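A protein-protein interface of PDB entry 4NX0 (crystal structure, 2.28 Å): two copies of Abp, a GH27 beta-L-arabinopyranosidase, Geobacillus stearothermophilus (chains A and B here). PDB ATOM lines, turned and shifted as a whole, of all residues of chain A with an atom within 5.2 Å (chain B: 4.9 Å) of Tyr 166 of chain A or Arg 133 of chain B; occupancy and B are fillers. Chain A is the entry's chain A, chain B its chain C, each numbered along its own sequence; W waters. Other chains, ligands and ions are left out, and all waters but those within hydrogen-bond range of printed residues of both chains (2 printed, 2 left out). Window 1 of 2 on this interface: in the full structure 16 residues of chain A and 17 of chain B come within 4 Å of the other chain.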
ATOM      1  N   ARG A 129     -26.103 -33.286 -28.603  1.00  0.00           N
ATOM      2  CA  ARG A 129     -25.725 -32.007 -29.121  1.00  0.00           C
ATOM      3  C   ARG A 129     -24.346 -31.622 -28.640  1.00  0.00           C
ATOM      4  O   ARG A 129     -24.030 -31.797 -27.436  1.00  0.00           O
ATOM      5  CB  ARG A 129     -26.707 -30.947 -28.573  1.00  0.00           C
ATOM      6  CG  ARG A 129     -26.389 -29.521 -29.002  1.00  0.00           C
ATOM      7  CD  ARG A 129     -27.271 -28.531 -28.220  1.00  0.00           C
ATOM      8  NE  ARG A 129     -27.052 -28.599 -26.772  1.00  0.00           N
ATOM      9  CZ  ARG A 129     -26.321 -27.741 -26.073  1.00  0.00           C
ATOM     10  NH1 ARG A 129     -25.733 -26.737 -26.687  1.00  0.00           N
ATOM     11  NH2 ARG A 129     -26.210 -27.851 -24.759  1.00  0.00           N
ATOM     12  N   GLY A 130     -23.570 -31.052 -29.554  1.00  0.00           N
ATOM     13  CA  GLY A 130     -22.320 -30.419 -29.190  1.00  0.00           C
ATOM     14  C   GLY A 130     -21.057 -31.164 -29.583  1.00  0.00           C
ATOM     15  O   GLY A 130     -21.034 -31.918 -30.554  1.00  0.00           O
ATOM     16  N   ILE A 131     -20.027 -30.905 -28.799  1.00  0.00           N
ATOM     17  CA  ILE A 131     -18.695 -31.431 -28.995  1.00  0.00           C
ATOM     18  C   ILE A 131     -18.187 -31.946 -27.649  1.00  0.00           C
ATOM     19  O   ILE A 131     -18.486 -31.365 -26.627  1.00  0.00           O
ATOM     20  CB  ILE A 131     -17.772 -30.380 -29.613  1.00  0.00           C
ATOM     21  CG1 ILE A 131     -16.417 -30.993 -29.993  1.00  0.00           C
ATOM     22  CG2 ILE A 131     -17.581 -29.165 -28.696  1.00  0.00           C
ATOM     23  CD1 ILE A 131     -15.596 -30.148 -30.949  1.00  0.00           C
ATOM     24  N   PRO A 132     -17.442 -33.054 -27.644  1.00  0.00           N
ATOM     25  CA  PRO A 132     -17.118 -33.627 -26.330  1.00  0.00           C
ATOM     26  C   PRO A 132     -16.300 -32.689 -25.464  1.00  0.00           C
ATOM     27  O   PRO A 132     -15.365 -32.044 -25.955  1.00  0.00           O
ATOM     28  CB  PRO A 132     -16.309 -34.870 -26.653  1.00  0.00           C
ATOM     29  CG  PRO A 132     -16.779 -35.246 -28.043  1.00  0.00           C
ATOM     30  CD  PRO A 132     -17.008 -33.904 -28.735  1.00  0.00           C
ATOM     31  N   ARG A 133     -16.620 -32.656 -24.174  1.00  0.00           N
ATOM     32  CA  ARG A 133     -15.780 -31.911 -23.244  1.00  0.00           C
ATOM     33  C   ARG A 133     -14.332 -32.310 -23.278  1.00  0.00           C
ATOM     34  O   ARG A 133     -13.458 -31.443 -23.262  1.00  0.00           O
ATOM     35  CB  ARG A 133     -16.317 -32.064 -21.810  1.00  0.00           C
ATOM     36  CG  ARG A 133     -17.757 -31.597 -21.643  1.00  0.00           C
ATOM     37  CD  ARG A 133     -18.092 -31.356 -20.197  1.00  0.00           C
ATOM     38  NE  ARG A 133     -19.495 -31.032 -20.008  1.00  0.00           N
ATOM     39  CZ  ARG A 133     -20.065 -30.840 -18.810  1.00  0.00           C
ATOM     40  NH1 ARG A 133     -19.339 -30.816 -17.699  1.00  0.00           N
ATOM     41  NH2 ARG A 133     -21.358 -30.678 -18.717  1.00  0.00           N
ATOM     42  N   VAL A 136     -12.575 -30.476 -26.047  1.00  0.00           N
ATOM     43  CA  VAL A 136     -12.399 -29.078 -25.774  1.00  0.00           C
ATOM     44  C   VAL A 136     -11.257 -28.864 -24.763  1.00  0.00           C
ATOM     45  O   VAL A 136     -10.382 -28.053 -24.997  1.00  0.00           O
ATOM     46  CB  VAL A 136     -13.690 -28.497 -25.243  1.00  0.00           C
ATOM     47  CG1 VAL A 136     -13.520 -27.094 -24.637  1.00  0.00           C
ATOM     48  CG2 VAL A 136     -14.698 -28.466 -26.378  1.00  0.00           C
ATOM     49  N   HIS A 137     -11.187 -29.692 -23.724  1.00  0.00           N
ATOM     50  CA  HIS A 137     -10.110 -29.600 -22.777  1.00  0.00           C
ATOM     51  C   HIS A 137      -8.760 -29.966 -23.354  1.00  0.00           C
ATOM     52  O   HIS A 137      -7.760 -29.340 -23.008  1.00  0.00           O
ATOM     53  CB  HIS A 137     -10.411 -30.372 -21.514  1.00  0.00           C
ATOM     54  CG  HIS A 137     -11.488 -29.689 -20.765  1.00  0.00           C
ATOM     55  ND1 HIS A 137     -11.306 -28.504 -20.063  1.00  0.00           N
ATOM     56  CD2 HIS A 137     -12.803 -29.949 -20.710  1.00  0.00           C
ATOM     57  CE1 HIS A 137     -12.468 -28.066 -19.608  1.00  0.00           C
ATOM     58  NE2 HIS A 137     -13.400 -28.909 -20.021  1.00  0.00           N
ATOM     59  N   ALA A 153     -16.193 -24.226 -28.968  1.00  0.00           N
ATOM     60  CA  ALA A 153     -17.125 -24.473 -27.916  1.00  0.00           C
ATOM     61  C   ALA A 153     -17.761 -23.218 -27.414  1.00  0.00           C
ATOM     62  O   ALA A 153     -17.107 -22.199 -27.297  1.00  0.00           O
ATOM     63  CB  ALA A 153     -16.424 -25.184 -26.763  1.00  0.00           C
ATOM     64  N   ASP A 154     -19.037 -23.325 -27.044  1.00  0.00           N
ATOM     65  CA  ASP A 154     -19.745 -22.305 -26.272  1.00  0.00           C
ATOM     66  C   ASP A 154     -19.194 -22.340 -24.860  1.00  0.00           C
ATOM     67  O   ASP A 154     -18.965 -23.431 -24.258  1.00  0.00           O
ATOM     68  CB  ASP A 154     -21.238 -22.584 -26.289  1.00  0.00           C
ATOM     69  CG  ASP A 154     -22.088 -21.382 -25.943  1.00  0.00           C
ATOM     70  OD1 ASP A 154     -21.929 -20.671 -24.845  1.00  0.00           O
ATOM     71  OD2 ASP A 154     -22.957 -21.128 -26.781  1.00  0.00           O
ATOM     72  N   THR A 155     -18.926 -21.169 -24.274  1.00  0.00           N
ATOM     73  CA  THR A 155     -18.402 -21.161 -22.889  1.00  0.00           C
ATOM     74  C   THR A 155     -19.479 -21.287 -21.847  1.00  0.00           C
ATOM     75  O   THR A 155     -19.185 -21.453 -20.684  1.00  0.00           O
ATOM     76  CB  THR A 155     -17.595 -19.892 -22.634  1.00  0.00           C
ATOM     77  OG1 THR A 155     -18.401 -18.745 -22.865  1.00  0.00           O
ATOM     78  CG2 THR A 155     -16.379 -19.779 -23.632  1.00  0.00           C
ATOM     79  N   SER A 157     -22.645 -23.444 -22.221  1.00  0.00           N
ATOM     80  CA  SER A 157     -23.670 -24.342 -22.745  1.00  0.00           C
ATOM     81  C   SER A 157     -23.349 -25.779 -22.411  1.00  0.00           C
ATOM     82  O   SER A 157     -22.338 -26.332 -22.879  1.00  0.00           O
ATOM     83  CB  SER A 157     -23.761 -24.194 -24.261  1.00  0.00           C
ATOM     84  OG  SER A 157     -24.937 -24.809 -24.777  1.00  0.00           O
ATOM     85  N   ILE A 158     -24.148 -26.347 -21.534  1.00  0.00           N
ATOM     86  CA  ILE A 158     -24.034 -27.726 -21.136  1.00  0.00           C
ATOM     87  C   ILE A 158     -25.405 -28.359 -21.190  1.00  0.00           C
ATOM     88  O   ILE A 158     -26.404 -27.660 -21.394  1.00  0.00           O
ATOM     89  CB  ILE A 158     -23.476 -27.899 -19.719  1.00  0.00           C
ATOM     90  CG1 ILE A 158     -24.338 -27.169 -18.697  1.00  0.00           C
ATOM     91  CG2 ILE A 158     -22.066 -27.378 -19.670  1.00  0.00           C
ATOM     92  CD1 ILE A 158     -24.070 -27.611 -17.268  1.00  0.00           C
ATOM     93  N   ASP A 164     -21.272 -35.226 -21.062  1.00  0.00           N
ATOM     94  CA  ASP A 164     -20.345 -35.655 -22.129  1.00  0.00           C
ATOM     95  C   ASP A 164     -19.851 -34.481 -22.988  1.00  0.00           C
ATOM     96  O   ASP A 164     -18.710 -34.508 -23.449  1.00  0.00           O
ATOM     97  CB  ASP A 164     -20.972 -36.711 -23.009  1.00  0.00           C
ATOM     98  CG  ASP A 164     -21.273 -38.018 -22.246  1.00  0.00           C
ATOM     99  OD1 ASP A 164     -20.656 -38.254 -21.185  1.00  0.00           O
ATOM    100  OD2 ASP A 164     -22.129 -38.791 -22.765  1.00  0.00           O
ATOM    101  N   MET A 165     -20.715 -33.520 -23.262  1.00  0.00           N
ATOM    102  CA  MET A 165     -20.480 -32.516 -24.299  1.00  0.00           C
ATOM    103  C   MET A 165     -20.533 -31.081 -23.767  1.00  0.00           C
ATOM    104  O   MET A 165     -21.053 -30.841 -22.656  1.00  0.00           O
ATOM    105  CB  MET A 165     -21.543 -32.596 -25.382  1.00  0.00           C
ATOM    106  CG  MET A 165     -21.961 -33.978 -25.839  1.00  0.00           C
ATOM    107  SD  MET A 165     -20.662 -34.936 -26.555  1.00  0.00           S
ATOM    108  CE  MET A 165     -20.800 -34.530 -28.312  1.00  0.00           C
ATOM    109  N   TYR A 166     -19.972 -30.164 -24.544  1.00  0.00           N
ATOM    110  CA  TYR A 166     -20.258 -28.769 -24.458  1.00  0.00           C
ATOM    111  C   TYR A 166     -20.955 -28.397 -25.770  1.00  0.00           C
ATOM    112  O   TYR A 166     -20.721 -28.974 -26.809  1.00  0.00           O
ATOM    113  CB  TYR A 166     -19.006 -27.929 -24.386  1.00  0.00           C
ATOM    114  CG  TYR A 166     -18.209 -28.055 -23.116  1.00  0.00           C
ATOM    115  CD1 TYR A 166     -18.803 -27.916 -21.897  1.00  0.00           C
ATOM    116  CD2 TYR A 166     -16.818 -28.304 -23.156  1.00  0.00           C
ATOM    117  CE1 TYR A 166     -18.047 -27.960 -20.744  1.00  0.00           C
ATOM    118  CE2 TYR A 166     -16.068 -28.375 -21.999  1.00  0.00           C
ATOM    119  CZ  TYR A 166     -16.667 -28.219 -20.799  1.00  0.00           C
ATOM    120  OH  TYR A 166     -15.996 -28.317 -19.641  1.00  0.00           O
ATOM    121  N   GLY A 167     -21.797 -27.401 -25.694  1.00  0.00           N
ATOM    122  CA  GLY A 167     -22.394 -26.860 -26.858  1.00  0.00           C
ATOM    123  C   GLY A 167     -21.363 -26.254 -27.788  1.00  0.00           C
ATOM    124  O   GLY A 167     -20.315 -25.799 -27.363  1.00  0.00           O
ATOM    125  N   VAL A 168     -21.694 -26.265 -29.086  1.00  0.00           N
ATOM    126  CA  VAL A 168     -20.952 -25.636 -30.113  1.00  0.00           C
ATOM    127  C   VAL A 168     -21.541 -24.256 -30.477  1.00  0.00           C
ATOM    128  O   VAL A 168     -22.768 -24.079 -30.630  1.00  0.00           O
ATOM    129  CB  VAL A 168     -20.946 -26.513 -31.343  1.00  0.00           C
ATOM    130  CG1 VAL A 168     -20.341 -25.795 -32.513  1.00  0.00           C
ATOM    131  CG2 VAL A 168     -20.119 -27.732 -31.063  1.00  0.00           C
ATOM    132  N   PHE B  82     -11.367 -22.749 -20.970  1.00  0.00           N
ATOM    133  CA  PHE B  82     -10.996 -24.134 -21.031  1.00  0.00           C
ATOM    134  C   PHE B  82      -9.517 -24.394 -21.061  1.00  0.00           C
ATOM    135  O   PHE B  82      -9.105 -25.407 -21.580  1.00  0.00           O
ATOM    136  CB  PHE B  82     -11.681 -24.829 -22.249  1.00  0.00           C
ATOM    137  CG  PHE B  82     -13.112 -24.569 -22.375  1.00  0.00           C
ATOM    138  CD1 PHE B  82     -13.999 -25.117 -21.458  1.00  0.00           C
ATOM    139  CD2 PHE B  82     -13.619 -23.928 -23.431  1.00  0.00           C
ATOM    140  CE1 PHE B  82     -15.376 -24.930 -21.573  1.00  0.00           C
ATOM    141  CE2 PHE B  82     -15.020 -23.737 -23.583  1.00  0.00           C
ATOM    142  CZ  PHE B  82     -15.882 -24.245 -22.648  1.00  0.00           C
ATOM    143  N   ILE B 131     -14.495 -26.570  -7.533  1.00  0.00           N
ATOM    144  CA  ILE B 131     -13.306 -27.368  -7.719  1.00  0.00           C
ATOM    145  C   ILE B 131     -12.968 -27.370  -9.208  1.00  0.00           C
ATOM    146  O   ILE B 131     -13.842 -27.330 -10.031  1.00  0.00           O
ATOM    147  CB  ILE B 131     -13.526 -28.761  -7.173  1.00  0.00           C
ATOM    148  CG1 ILE B 131     -12.245 -29.554  -7.202  1.00  0.00           C
ATOM    149  CG2 ILE B 131     -14.622 -29.536  -7.936  1.00  0.00           C
ATOM    150  CD1 ILE B 131     -12.270 -30.779  -6.294  1.00  0.00           C
ATOM    151  N   PRO B 132     -11.687 -27.368  -9.567  1.00  0.00           N
ATOM    152  CA  PRO B 132     -11.372 -27.145 -10.969  1.00  0.00           C
ATOM    153  C   PRO B 132     -11.866 -28.227 -11.836  1.00  0.00           C
ATOM    154  O   PRO B 132     -11.834 -29.431 -11.458  1.00  0.00           O
ATOM    155  CB  PRO B 132      -9.861 -27.104 -11.005  1.00  0.00           C
ATOM    156  CG  PRO B 132      -9.448 -26.645  -9.640  1.00  0.00           C
ATOM    157  CD  PRO B 132     -10.474 -27.290  -8.711  1.00  0.00           C
ATOM    158  N   ARG B 133     -12.378 -27.843 -13.016  1.00  0.00           N
ATOM    159  CA  ARG B 133     -12.837 -28.872 -13.951  1.00  0.00           C
ATOM    160  C   ARG B 133     -11.743 -29.884 -14.232  1.00  0.00           C
ATOM    161  O   ARG B 133     -11.982 -31.077 -14.362  1.00  0.00           O
ATOM    162  CB  ARG B 133     -13.310 -28.197 -15.222  1.00  0.00           C
ATOM    163  CG  ARG B 133     -14.475 -27.265 -15.011  1.00  0.00           C
ATOM    164  CD  ARG B 133     -15.200 -26.956 -16.305  1.00  0.00           C
ATOM    165  NE  ARG B 133     -16.249 -25.977 -16.087  1.00  0.00           N
ATOM    166  CZ  ARG B 133     -17.003 -25.480 -17.063  1.00  0.00           C
ATOM    167  NH1 ARG B 133     -16.899 -25.938 -18.297  1.00  0.00           N
ATOM    168  NH2 ARG B 133     -17.847 -24.519 -16.820  1.00  0.00           N
ATOM    169  N   GLN B 134     -10.514 -29.410 -14.384  1.00  0.00           N
ATOM    170  CA  GLN B 134      -9.432 -30.335 -14.747  1.00  0.00           C
ATOM    171  C   GLN B 134      -9.200 -31.327 -13.643  1.00  0.00           C
ATOM    172  O   GLN B 134      -8.786 -32.444 -13.904  1.00  0.00           O
ATOM    173  CB  GLN B 134      -8.133 -29.587 -15.110  1.00  0.00           C
ATOM    174  CG  GLN B 134      -7.565 -28.821 -13.923  1.00  0.00           C
ATOM    175  CD  GLN B 134      -6.343 -27.961 -14.287  1.00  0.00           C
ATOM    176  OE1 GLN B 134      -6.241 -27.475 -15.376  1.00  0.00           O
ATOM    177  NE2 GLN B 134      -5.478 -27.716 -13.303  1.00  0.00           N
ATOM    178  N   ALA B 135      -9.468 -30.963 -12.393  1.00  0.00           N
ATOM    179  CA  ALA B 135      -9.293 -31.931 -11.301  1.00  0.00           C
ATOM    180  C   ALA B 135     -10.340 -33.004 -11.340  1.00  0.00           C
ATOM    181  O   ALA B 135     -10.067 -34.187 -11.099  1.00  0.00           O
ATOM    182  CB  ALA B 135      -9.354 -31.255  -9.963  1.00  0.00           C
ATOM    183  N   VAL B 136     -11.541 -32.619 -11.729  1.00  0.00           N
ATOM    184  CA  VAL B 136     -12.650 -33.563 -11.836  1.00  0.00           C
ATOM    185  C   VAL B 136     -12.385 -34.516 -13.009  1.00  0.00           C
ATOM    186  O   VAL B 136     -12.617 -35.707 -12.857  1.00  0.00           O
ATOM    187  CB  VAL B 136     -13.946 -32.800 -11.980  1.00  0.00           C
ATOM    188  CG1 VAL B 136     -15.146 -33.681 -12.406  1.00  0.00           C
ATOM    189  CG2 VAL B 136     -14.255 -32.120 -10.687  1.00  0.00           C
ATOM    190  N   HIS B 137     -11.874 -34.013 -14.110  1.00  0.00           N
ATOM    191  CA  HIS B 137     -11.625 -34.842 -15.294  1.00  0.00           C
ATOM    192  C   HIS B 137     -10.471 -35.783 -15.146  1.00  0.00           C
ATOM    193  O   HIS B 137     -10.590 -36.913 -15.510  1.00  0.00           O
ATOM    194  CB  HIS B 137     -11.384 -33.997 -16.539  1.00  0.00           C
ATOM    195  CG  HIS B 137     -12.488 -33.044 -16.880  1.00  0.00           C
ATOM    196  ND1 HIS B 137     -12.177 -31.829 -17.435  1.00  0.00           N
ATOM    197  CD2 HIS B 137     -13.832 -33.053 -16.713  1.00  0.00           C
ATOM    198  CE1 HIS B 137     -13.283 -31.146 -17.636  1.00  0.00           C
ATOM    199  NE2 HIS B 137     -14.297 -31.852 -17.175  1.00  0.00           N
ATOM    200  N   ILE B 158     -22.106 -24.992 -12.889  1.00  0.00           N
ATOM    201  CA  ILE B 158     -21.051 -24.268 -13.479  1.00  0.00           C
ATOM    202  C   ILE B 158     -21.250 -22.795 -13.195  1.00  0.00           C
ATOM    203  O   ILE B 158     -22.295 -22.398 -12.702  1.00  0.00           O
ATOM    204  CB  ILE B 158     -20.969 -24.472 -14.980  1.00  0.00           C
ATOM    205  CG1 ILE B 158     -22.273 -24.049 -15.680  1.00  0.00           C
ATOM    206  CG2 ILE B 158     -20.703 -25.936 -15.310  1.00  0.00           C
ATOM    207  CD1 ILE B 158     -22.117 -23.910 -17.194  1.00  0.00           C
ATOM    208  N   CYS B 159     -20.251 -22.006 -13.555  1.00  0.00           N
ATOM    209  CA  CYS B 159     -20.361 -20.552 -13.591  1.00  0.00           C
ATOM    210  C   CYS B 159     -20.688 -20.219 -15.043  1.00  0.00           C
ATOM    211  O   CYS B 159     -20.012 -20.675 -15.955  1.00  0.00           O
ATOM    212  CB  CYS B 159     -19.049 -19.931 -13.213  1.00  0.00           C
ATOM    213  SG  CYS B 159     -19.050 -18.143 -13.406  1.00  0.00           S
ATOM    214  N   ASN B 162     -17.463 -18.043 -16.516  1.00  0.00           N
ATOM    215  CA  ASN B 162     -16.103 -18.516 -16.390  1.00  0.00           C
ATOM    216  C   ASN B 162     -16.074 -20.057 -16.335  1.00  0.00           C
ATOM    217  O   ASN B 162     -16.899 -20.662 -15.638  1.00  0.00           O
ATOM    218  CB  ASN B 162     -15.512 -17.912 -15.114  1.00  0.00           C
ATOM    219  CG  ASN B 162     -14.215 -18.542 -14.685  1.00  0.00           C
ATOM    220  OD1 ASN B 162     -14.179 -19.634 -14.130  1.00  0.00           O
ATOM    221  ND2 ASN B 162     -13.105 -17.883 -15.019  1.00  0.00           N
ATOM    222  N   THR B 163     -15.115 -20.659 -17.042  1.00  0.00           N
ATOM    223  CA  THR B 163     -15.085 -22.099 -17.269  1.00  0.00           C
ATOM    224  C   THR B 163     -14.147 -22.892 -16.348  1.00  0.00           C
ATOM    225  O   THR B 163     -13.982 -24.099 -16.552  1.00  0.00           O
ATOM    226  CB  THR B 163     -14.641 -22.390 -18.691  1.00  0.00           C
ATOM    227  OG1 THR B 163     -13.334 -21.871 -18.926  1.00  0.00           O
ATOM    228  CG2 THR B 163     -15.601 -21.786 -19.692  1.00  0.00           C
ATOM    229  N   ASP B 164     -13.565 -22.255 -15.336  1.00  0.00           N
ATOM    230  CA  ASP B 164     -12.501 -22.890 -14.580  1.00  0.00           C
ATOM    231  C   ASP B 164     -12.928 -24.007 -13.650  1.00  0.00           C
ATOM    232  O   ASP B 164     -12.210 -25.017 -13.530  1.00  0.00           O
ATOM    233  CB  ASP B 164     -11.739 -21.855 -13.778  1.00  0.00           C
ATOM    234  CG  ASP B 164     -10.992 -20.846 -14.655  1.00  0.00           C
ATOM    235  OD1 ASP B 164     -10.800 -21.122 -15.891  1.00  0.00           O
ATOM    236  OD2 ASP B 164     -10.704 -19.747 -14.100  1.00  0.00           O
ATOM    237  N   MET B 165     -14.120 -23.894 -13.043  1.00  0.00           N
ATOM    238  CA  MET B 165     -14.547 -24.827 -11.991  1.00  0.00           C
ATOM    239  C   MET B 165     -15.865 -25.552 -12.303  1.00  0.00           C
ATOM    240  O   MET B 165     -16.613 -25.137 -13.184  1.00  0.00           O
ATOM    241  CB  MET B 165     -14.798 -24.024 -10.722  1.00  0.00           C
ATOM    242  CG  MET B 165     -13.763 -22.935 -10.421  1.00  0.00           C
ATOM    243  SD  MET B 165     -12.134 -23.525 -10.172  1.00  0.00           S
ATOM    244  CE  MET B 165     -12.062 -23.808  -8.422  1.00  0.00           C
ATOM    245  N   TYR B 166     -16.134 -26.602 -11.521  1.00  0.00           N
ATOM    246  CA  TYR B 166     -17.432 -27.167 -11.296  1.00  0.00           C
ATOM    247  C   TYR B 166     -17.778 -26.971  -9.871  1.00  0.00           C
ATOM    248  O   TYR B 166     -16.907 -26.876  -8.996  1.00  0.00           O
ATOM    249  CB  TYR B 166     -17.454 -28.678 -11.544  1.00  0.00           C
ATOM    250  CG  TYR B 166     -17.230 -29.168 -12.949  1.00  0.00           C
ATOM    251  CD1 TYR B 166     -17.939 -28.629 -13.977  1.00  0.00           C
ATOM    252  CD2 TYR B 166     -16.257 -30.111 -13.251  1.00  0.00           C
ATOM    253  CE1 TYR B 166     -17.749 -29.072 -15.315  1.00  0.00           C
ATOM    254  CE2 TYR B 166     -16.041 -30.534 -14.549  1.00  0.00           C
ATOM    255  CZ  TYR B 166     -16.812 -30.010 -15.587  1.00  0.00           C
ATOM    256  OH  TYR B 166     -16.622 -30.425 -16.860  1.00  0.00           O
HETATM  257  O   HOH W   1     -17.449 -18.324 -19.748  1.00  0.00           O
HETATM  258  O   HOH W   2     -18.891 -24.317 -19.798  1.00  0.00           O
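The guanidinium group (NH1) of Arg 133 of chain B lies within hydrogen-bond range of the side-chain hydroxyl (OH) of Tyr 166 of chain A (2.9 Å). The guanidinium group (NH1) of Arg 133 of chain A lies within hydrogen-bond range of the side-chain hydroxyl (OH) of Tyr 166 of chain B (2.9 Å).
The guanidinium group (NE) of Arg 133 of chain B sits at hydrogen-bond distance from the backbone carbonyl oxygen (O) of Met 165 of chain B, 3.0 Å away. A ring nitrogen (NE2) of His 137 of chain B lies within hydrogen-bond range of the side-chain hydroxyl (OH) of Tyr 166 of chain B (2.7 Å). The backbone NH (N) of Phe 82 of chain B sits at hydrogen-bond distance from the side-chain hydroxyl (OG1) of Thr 163 of chain B (3.0 Å). The backbone NH of Tyr 166 of chain A is in hydrogen-bond range of the backbone carbonyl oxygen of Ile 131 of chain A (2.8 Å). O of Thr 163 of chain B lies within hydrogen-bond range of NE of Arg 133 of chain B (3.0 Å). O of Asp 164 of chain A is in hydrogen-bond range of N of Arg 133 of chain A (2.9 Å).
CG1 of Val 136 of chain A touches CD2 of Phe 82 of chain B (3.4 Å). CE1 of His 137 of chain A touches CD1 of Phe 82 of chain B, at 3.8 Å. CE1 of His 137 of chain B touches NE2 of His 137 of chain A, 3.3 Å away. Ala 153 of chain A touches Phe 82 of chain B (CB to CE2, 3.8 Å). Phe 82 of chain B touches Asp 154 of chain A. Thr 155 of chain A touches Phe 82 of chain B (CA to CZ, 3.99 Å). Thr 155 of chain A touches Thr 163 of chain B (O to CG2, 3.7 Å). Tyr 166 of chain A touches Phe 82 of chain B (CE2 to CE1, 3.5 Å). Tyr 166 of chain B touches Tyr 166 of chain A (OH to OH, 3.5 Å).
Of chain B, only Phe 82 (3.5 Å), Arg 133 (2.9 Å) and Tyr 166 (3.5 Å) come within 4 Å of Tyr 166 of chain A. Printed residues of chain A within 4 Å of Phe 82 of chain B: Val 136 (3.4 Å), His 137 (3.8 Å), Ala 153 (3.8 Å), Asp 154 (3.6 Å), Thr 155 (3.99 Å) and Tyr 166 (3.5 Å). Printed residues of chain B within 4 Å of His 137 of chain A: Phe 82 (3.8 Å) and His 137 (3.3 Å). Printed residues of chain B within 4 Å of Asp 154 of chain A: Phe 82. Val 168 of chain A touches none of the printed residues of chain B. The nearest residue of chain B that does not touch Tyr 166 of chain A is His 137 of chain B (4.4 Å). The nearest printed residue of chain B that does not touch Ala 153 of chain A is Thr 163 of chain B (7.8 Å).
Of the 15 printed residues of chain B, 5 touch a printed residue of chain A. Hydrophobic or aromatic side chains of chain B that line the printed part of chain A: Phe 82, His 137 and Tyr 166. Among the printed residues, 11 pairs touch across the chains. Among the printed residues, no Asp or Glu carboxylate lies within 4 Å of a Lys or Arg side-chain nitrogen of the other chain.
Arg 133 of chain A touches Tyr 166 of chain B, and with the chains exchanged Tyr 166 of chain A touches Arg 133 of chain B. His 137 of chain B touches its own counterpart, His 137 of chain A. Tyr 166 of chain A touches its own counterpart, Tyr 166 of chain B. Positions printed for both chains: 131, 132, 133, 136, 137, 158, 164, 165 and 166. Of the 11 pairs that touch across the chains among the printed residues, 4 have their exchanged pair printed and touching as well.
Water W2 lies within hydrogen-bond range of NH1 of Arg 133 of chain B (3.0 Å) and O of Thr 155 of chain A (3.0 Å). Water W1 lies within hydrogen-bond range of the backbone NH (N) of Asn 162 of chain B (3.2 Å) and the side-chain hydroxyl (OG1) of Thr 155 of chain A (3.3 Å).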
